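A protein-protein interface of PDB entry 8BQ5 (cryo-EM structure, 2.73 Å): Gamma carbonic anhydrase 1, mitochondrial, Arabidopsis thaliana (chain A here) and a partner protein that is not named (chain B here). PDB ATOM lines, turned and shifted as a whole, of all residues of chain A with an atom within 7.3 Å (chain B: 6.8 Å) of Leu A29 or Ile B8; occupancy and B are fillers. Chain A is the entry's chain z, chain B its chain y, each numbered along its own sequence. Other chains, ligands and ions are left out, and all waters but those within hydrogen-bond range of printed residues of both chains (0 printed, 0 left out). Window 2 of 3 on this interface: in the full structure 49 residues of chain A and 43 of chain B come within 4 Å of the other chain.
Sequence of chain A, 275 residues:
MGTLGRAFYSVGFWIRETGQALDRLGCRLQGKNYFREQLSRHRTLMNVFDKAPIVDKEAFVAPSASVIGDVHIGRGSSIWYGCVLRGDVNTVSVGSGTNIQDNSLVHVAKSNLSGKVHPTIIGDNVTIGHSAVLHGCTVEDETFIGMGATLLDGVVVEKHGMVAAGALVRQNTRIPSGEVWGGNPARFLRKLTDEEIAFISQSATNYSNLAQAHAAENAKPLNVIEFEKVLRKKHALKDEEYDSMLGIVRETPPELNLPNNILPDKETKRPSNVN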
ATOM      1  N   ASP A  23      12.326  11.136  20.713  1.00  0.00           N
ATOM      2  CA  ASP A  23      11.640   9.849  20.759  1.00  0.00           C
ATOM      3  C   ASP A  23      12.437   8.777  20.024  1.00  0.00           C
ATOM      4  O   ASP A  23      12.512   7.627  20.472  1.00  0.00           O
ATOM      5  CB  ASP A  23      10.237   9.984  20.169  1.00  0.00           C
ATOM      6  CG  ASP A  23       9.450   8.694  20.243  1.00  0.00           C
ATOM      7  OD1 ASP A  23       9.632   7.830  19.361  1.00  0.00           O
ATOM      8  OD2 ASP A  23       8.647   8.544  21.186  1.00  0.00           O
ATOM      9  N   ARG A  24      13.036   9.139  18.888  1.00  0.00           N
ATOM     10  CA  ARG A  24      13.863   8.186  18.153  1.00  0.00           C
ATOM     11  C   ARG A  24      15.084   7.769  18.967  1.00  0.00           C
ATOM     12  O   ARG A  24      15.473   6.595  18.961  1.00  0.00           O
ATOM     13  CB  ARG A  24      14.278   8.787  16.811  1.00  0.00           C
ATOM     14  CG  ARG A  24      13.190   8.703  15.753  1.00  0.00           C
ATOM     15  CD  ARG A  24      13.743   8.928  14.361  1.00  0.00           C
ATOM     16  NE  ARG A  24      14.482  10.179  14.258  1.00  0.00           N
ATOM     17  CZ  ARG A  24      13.920  11.373  14.141  1.00  0.00           C
ATOM     18  NH1 ARG A  24      12.606  11.519  14.115  1.00  0.00           N
ATOM     19  NH2 ARG A  24      14.695  12.449  14.044  1.00  0.00           N
ATOM     20  N   LEU A  25      15.705   8.720  19.669  1.00  0.00           N
ATOM     21  CA  LEU A  25      16.811   8.390  20.567  1.00  0.00           C
ATOM     22  C   LEU A  25      16.368   7.407  21.643  1.00  0.00           C
ATOM     23  O   LEU A  25      17.052   6.411  21.922  1.00  0.00           O
ATOM     24  CB  LEU A  25      17.364   9.665  21.208  1.00  0.00           C
ATOM     25  CG  LEU A  25      18.434   9.477  22.289  1.00  0.00           C
ATOM     26  CD1 LEU A  25      19.625   8.703  21.752  1.00  0.00           C
ATOM     27  CD2 LEU A  25      18.877  10.810  22.878  1.00  0.00           C
ATOM     28  N   GLY A  26      15.215   7.676  22.258  1.00  0.00           N
ATOM     29  CA  GLY A  26      14.703   6.771  23.272  1.00  0.00           C
ATOM     30  C   GLY A  26      14.460   5.372  22.738  1.00  0.00           C
ATOM     31  O   GLY A  26      14.779   4.382  23.397  1.00  0.00           O
ATOM     32  N   CYS A  27      13.934   5.237  21.522  1.00  0.00           N
ATOM     33  CA  CYS A  27      13.741   3.887  20.918  1.00  0.00           C
ATOM     34  C   CYS A  27      15.082   3.205  20.620  1.00  0.00           C
ATOM     35  O   CYS A  27      15.157   1.989  20.820  1.00  0.00           O
ATOM     36  CB  CYS A  27      12.972   3.971  19.607  1.00  0.00           C
ATOM     37  SG  CYS A  27      11.367   4.796  19.741  1.00  0.00           S
ATOM     38  N   ARG A  28      16.066   3.952  20.113  1.00  0.00           N
ATOM     39  CA  ARG A  28      17.412   3.403  19.802  1.00  0.00           C
ATOM     40  C   ARG A  28      18.062   2.883  21.090  1.00  0.00           C
ATOM     41  O   ARG A  28      18.710   1.833  21.009  1.00  0.00           O
ATOM     42  CB  ARG A  28      18.269   4.462  19.101  1.00  0.00           C
ATOM     43  CG  ARG A  28      18.179   4.428  17.584  1.00  0.00           C
ATOM     44  CD  ARG A  28      19.090   5.450  16.935  1.00  0.00           C
ATOM     45  NE  ARG A  28      18.614   5.876  15.626  1.00  0.00           N
ATOM     46  CZ  ARG A  28      18.116   7.076  15.355  1.00  0.00           C
ATOM     47  NH1 ARG A  28      18.021   7.990  16.304  1.00  0.00           N
ATOM     48  NH2 ARG A  28      17.713   7.361  14.131  1.00  0.00           N
ATOM     49  N   LEU A  29      17.848   3.553  22.236  1.00  0.00           N
ATOM     50  CA  LEU A  29      18.377   3.010  23.485  1.00  0.00           C
ATOM     51  C   LEU A  29      17.740   1.671  23.836  1.00  0.00           C
ATOM     52  O   LEU A  29      18.394   0.814  24.440  1.00  0.00           O
ATOM     53  CB  LEU A  29      18.173   4.002  24.629  1.00  0.00           C
ATOM     54  CG  LEU A  29      18.977   5.296  24.542  1.00  0.00           C
ATOM     55  CD1 LEU A  29      18.699   6.166  25.751  1.00  0.00           C
ATOM     56  CD2 LEU A  29      20.458   4.984  24.435  1.00  0.00           C
ATOM     57  N   GLN A  30      16.477   1.468  23.465  1.00  0.00           N
ATOM     58  CA  GLN A  30      15.759   0.208  23.791  1.00  0.00           C
ATOM     59  C   GLN A  30      15.884  -0.824  22.659  1.00  0.00           C
ATOM     60  O   GLN A  30      15.225  -1.875  22.758  1.00  0.00           O
ATOM     61  CB  GLN A  30      14.300   0.546  24.087  1.00  0.00           C
ATOM     62  CG  GLN A  30      14.144   1.564  25.202  1.00  0.00           C
ATOM     63  CD  GLN A  30      12.705   1.964  25.391  1.00  0.00           C
ATOM     64  OE1 GLN A  30      12.008   2.323  24.448  1.00  0.00           O
ATOM     65  NE2 GLN A  30      12.250   1.903  26.627  1.00  0.00           N
ATOM     66  N   GLY A  31      16.680  -0.546  21.621  1.00  0.00           N
ATOM     67  CA  GLY A  31      16.863  -1.481  20.492  1.00  0.00           C
ATOM     68  C   GLY A  31      15.639  -1.625  19.592  1.00  0.00           C
ATOM     69  O   GLY A  31      15.462  -2.712  19.025  1.00  0.00           O
ATOM     70  N   LYS A  32      14.834  -0.573  19.455  1.00  0.00           N
ATOM     71  CA  LYS A  32      13.658  -0.606  18.542  1.00  0.00           C
ATOM     72  C   LYS A  32      14.001   0.178  17.271  1.00  0.00           C
ATOM     73  O   LYS A  32      14.585   1.262  17.400  1.00  0.00           O
ATOM     74  CB  LYS A  32      12.416  -0.043  19.237  1.00  0.00           C
ATOM     75  CG  LYS A  32      11.986  -0.767  20.504  1.00  0.00           C
ATOM     76  CD  LYS A  32      11.376   0.158  21.528  1.00  0.00           C
ATOM     77  CE  LYS A  32      10.529  -0.568  22.549  1.00  0.00           C
ATOM     78  NZ  LYS A  32       9.182   0.034  22.666  1.00  0.00           N
ATOM     79  N   PHE A  35      10.699   2.733  13.821  1.00  0.00           N
ATOM     80  CA  PHE A  35      10.576   4.125  13.318  1.00  0.00           C
ATOM     81  C   PHE A  35      11.176   4.217  11.912  1.00  0.00           C
ATOM     82  O   PHE A  35      10.908   5.202  11.211  1.00  0.00           O
ATOM     83  CB  PHE A  35      11.214   5.114  14.297  1.00  0.00           C
ATOM     84  CG  PHE A  35      12.662   4.886  14.644  1.00  0.00           C
ATOM     85  CD1 PHE A  35      13.675   5.330  13.810  1.00  0.00           C
ATOM     86  CD2 PHE A  35      13.013   4.272  15.833  1.00  0.00           C
ATOM     87  CE1 PHE A  35      15.005   5.133  14.138  1.00  0.00           C
ATOM     88  CE2 PHE A  35      14.344   4.083  16.163  1.00  0.00           C
ATOM     89  CZ  PHE A  35      15.336   4.502  15.311  1.00  0.00           C
ATOM     90  N   THR B   3      21.163  -5.702  34.796  1.00  0.00           N
ATOM     91  CA  THR B   3      20.791  -4.463  35.474  1.00  0.00           C
ATOM     92  C   THR B   3      21.045  -3.251  34.587  1.00  0.00           C
ATOM     93  O   THR B   3      20.226  -2.323  34.536  1.00  0.00           O
ATOM     94  CB  THR B   3      21.561  -4.340  36.789  1.00  0.00           C
ATOM     95  OG1 THR B   3      21.185  -5.409  37.664  1.00  0.00           O
ATOM     96  CG2 THR B   3      21.252  -3.014  37.468  1.00  0.00           C
ATOM     97  N   LEU B   4      22.176  -3.241  33.881  1.00  0.00           N
ATOM     98  CA  LEU B   4      22.499  -2.121  33.003  1.00  0.00           C
ATOM     99  C   LEU B   4      21.499  -2.008  31.858  1.00  0.00           C
ATOM    100  O   LEU B   4      21.081  -0.901  31.493  1.00  0.00           O
ATOM    101  CB  LEU B   4      23.919  -2.281  32.464  1.00  0.00           C
ATOM    102  CG  LEU B   4      24.392  -1.178  31.523  1.00  0.00           C
ATOM    103  CD1 LEU B   4      24.332   0.154  32.241  1.00  0.00           C
ATOM    104  CD2 LEU B   4      25.800  -1.469  31.034  1.00  0.00           C
ATOM    105  N   GLY B   5      21.110  -3.145  31.277  1.00  0.00           N
ATOM    106  CA  GLY B   5      20.118  -3.118  30.216  1.00  0.00           C
ATOM    107  C   GLY B   5      18.788  -2.559  30.681  1.00  0.00           C
ATOM    108  O   GLY B   5      18.179  -1.727  30.004  1.00  0.00           O
ATOM    109  N   ARG B   6      18.326  -3.000  31.854  1.00  0.00           N
ATOM    110  CA  ARG B   6      17.073  -2.486  32.402  1.00  0.00           C
ATOM    111  C   ARG B   6      17.164  -0.996  32.700  1.00  0.00           C
ATOM    112  O   ARG B   6      16.212  -0.245  32.446  1.00  0.00           O
ATOM    113  CB  ARG B   6      16.699  -3.251  33.668  1.00  0.00           C
ATOM    114  CG  ARG B   6      16.328  -4.696  33.445  1.00  0.00           C
ATOM    115  CD  ARG B   6      15.467  -5.189  34.590  1.00  0.00           C
ATOM    116  NE  ARG B   6      16.199  -5.205  35.851  1.00  0.00           N
ATOM    117  CZ  ARG B   6      17.187  -6.041  36.141  1.00  0.00           C
ATOM    118  NH1 ARG B   6      17.571  -6.979  35.290  1.00  0.00           N
ATOM    119  NH2 ARG B   6      17.797  -5.939  37.318  1.00  0.00           N
ATOM    120  N   ALA B   7      18.291  -0.551  33.260  1.00  0.00           N
ATOM    121  CA  ALA B   7      18.449   0.869  33.554  1.00  0.00           C
ATOM    122  C   ALA B   7      18.394   1.702  32.280  1.00  0.00           C
ATOM    123  O   ALA B   7      17.725   2.743  32.234  1.00  0.00           O
ATOM    124  CB  ALA B   7      19.763   1.109  34.297  1.00  0.00           C
ATOM    125  N   ILE B   8      19.084   1.253  31.229  1.00  0.00           N
ATOM    126  CA  ILE B   8      19.075   1.996  29.975  1.00  0.00           C
ATOM    127  C   ILE B   8      17.688   1.965  29.344  1.00  0.00           C
ATOM    128  O   ILE B   8      17.248   2.946  28.734  1.00  0.00           O
ATOM    129  CB  ILE B   8      20.161   1.452  29.030  1.00  0.00           C
ATOM    130  CG1 ILE B   8      21.546   1.861  29.535  1.00  0.00           C
ATOM    131  CG2 ILE B   8      19.945   1.939  27.602  1.00  0.00           C
ATOM    132  CD1 ILE B   8      22.683   1.130  28.877  1.00  0.00           C
ATOM    133  N   TYR B   9      16.981   0.846  29.503  1.00  0.00           N
ATOM    134  CA  TYR B   9      15.593   0.738  28.986  1.00  0.00           C
ATOM    135  C   TYR B   9      14.709   1.777  29.690  1.00  0.00           C
ATOM    136  O   TYR B   9      13.957   2.468  28.991  1.00  0.00           O
ATOM    137  CB  TYR B   9      15.077  -0.692  29.149  1.00  0.00           C
ATOM    138  CG  TYR B   9      13.844  -1.026  28.354  1.00  0.00           C
ATOM    139  CD1 TYR B   9      12.579  -0.747  28.844  1.00  0.00           C
ATOM    140  CD2 TYR B   9      13.940  -1.644  27.120  1.00  0.00           C
ATOM    141  CE1 TYR B   9      11.441  -1.053  28.119  1.00  0.00           C
ATOM    142  CE2 TYR B   9      12.813  -1.960  26.382  1.00  0.00           C
ATOM    143  CZ  TYR B   9      11.560  -1.660  26.883  1.00  0.00           C
ATOM    144  OH  TYR B   9      10.445  -1.972  26.163  1.00  0.00           O
ATOM    145  N   THR B  10      14.808   1.894  31.019  1.00  0.00           N
ATOM    146  CA  THR B  10      13.996   2.860  31.755  1.00  0.00           C
ATOM    147  C   THR B  10      14.349   4.291  31.360  1.00  0.00           C
ATOM    148  O   THR B  10      13.462   5.146  31.199  1.00  0.00           O
ATOM    149  CB  THR B  10      14.182   2.655  33.257  1.00  0.00           C
ATOM    150  OG1 THR B  10      13.677   1.367  33.628  1.00  0.00           O
ATOM    151  CG2 THR B  10      13.436   3.715  34.037  1.00  0.00           C
ATOM    152  N   VAL B  11      15.643   4.570  31.193  1.00  0.00           N
ATOM    153  CA  VAL B  11      16.053   5.905  30.772  1.00  0.00           C
ATOM    154  C   VAL B  11      15.496   6.216  29.388  1.00  0.00           C
ATOM    155  O   VAL B  11      15.018   7.329  29.130  1.00  0.00           O
ATOM    156  CB  VAL B  11      17.586   6.029  30.816  1.00  0.00           C
ATOM    157  CG1 VAL B  11      18.026   7.306  30.137  1.00  0.00           C
ATOM    158  CG2 VAL B  11      18.075   5.992  32.255  1.00  0.00           C
ATOM    159  N   GLY B  12      15.535   5.237  28.482  1.00  0.00           N
ATOM    160  CA  GLY B  12      14.952   5.434  27.166  1.00  0.00           C
ATOM    161  C   GLY B  12      13.457   5.676  27.220  1.00  0.00           C
ATOM    162  O   GLY B  12      12.919   6.455  26.432  1.00  0.00           O
ATOM    163  N   ASN B  13      12.765   5.006  28.141  1.00  0.00           N
ATOM    164  CA  ASN B  13      11.340   5.267  28.331  1.00  0.00           C
ATOM    165  C   ASN B  13      11.100   6.717  28.734  1.00  0.00           C
ATOM    166  O   ASN B  13      10.211   7.391  28.194  1.00  0.00           O
ATOM    167  CB  ASN B  13      10.773   4.320  29.386  1.00  0.00           C
ATOM    168  CG  ASN B  13      10.059   3.137  28.780  1.00  0.00           C
ATOM    169  OD1 ASN B  13       9.885   3.060  27.566  1.00  0.00           O
ATOM    170  ND2 ASN B  13       9.649   2.200  29.623  1.00  0.00           N
ATOM    171  N   ILE B  15      13.053   9.214  28.088  1.00  0.00           N
ATOM    172  CA  ILE B  15      13.416  10.050  26.946  1.00  0.00           C
ATOM    173  C   ILE B  15      12.290  10.082  25.918  1.00  0.00           C
ATOM    174  O   ILE B  15      11.985  11.134  25.345  1.00  0.00           O
ATOM    175  CB  ILE B  15      14.742   9.563  26.334  1.00  0.00           C
ATOM    176  CG1 ILE B  15      15.886   9.770  27.329  1.00  0.00           C
ATOM    177  CG2 ILE B  15      15.038  10.289  25.032  1.00  0.00           C
ATOM    178  CD1 ILE B  15      17.233   9.339  26.813  1.00  0.00           C
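Of the printed residues of chain B, Leu A29 touches Ile B8 (3.7 Å) and Ile B15 (3.7 Å). Of chain A, only Leu A29 comes within 4 Å of Ile B8. No residue of chain A comes within 4 Å of Ala B7. Of the printed residues of chain A, Tyr B9 touches Gln A30 and Lys A32. Of the printed residues of chain A, Asn B13 touches Gln A30. Of the printed residues of chain B, Gly A26 touches Gly B12 and Ile B15. Printed residues of chain B within 4 Å of Gln A30: Tyr B9 and Asn B13. Asp A23 touches none of the printed residues of chain B. The nearest residue of chain A that does not touch Ile B8 is Gln A30 (4.9 Å).
NE2 of Gln A30 lies within hydrogen-bond range of O of Tyr B9 (3.0 Å). OD1 of Asn B13 lies within hydrogen-bond range of NE2 of Gln A30 (2.8 Å).
Of the 12 printed residues of chain B, 5 touch a printed residue of chain A. Among the printed residues, 7 pairs touch across the chains. Among the printed residues, no Asp or Glu carboxylate lies within 4 Å of a Lys or Arg side-chain nitrogen of the other chain.
The backbone carbonyl oxygen (O) of Cys A27 sits at hydrogen-bond distance from the backbone NH (N) of Lys A32 (2.9 Å).
Among the printed residues, pairs that only touch across the chains: Gly A26 with Gly B12, Leu A29 with Ile B15, Leu A29 with Ile B8, Gly A26 with Ile B15 and Lys A32 with Tyr B9.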
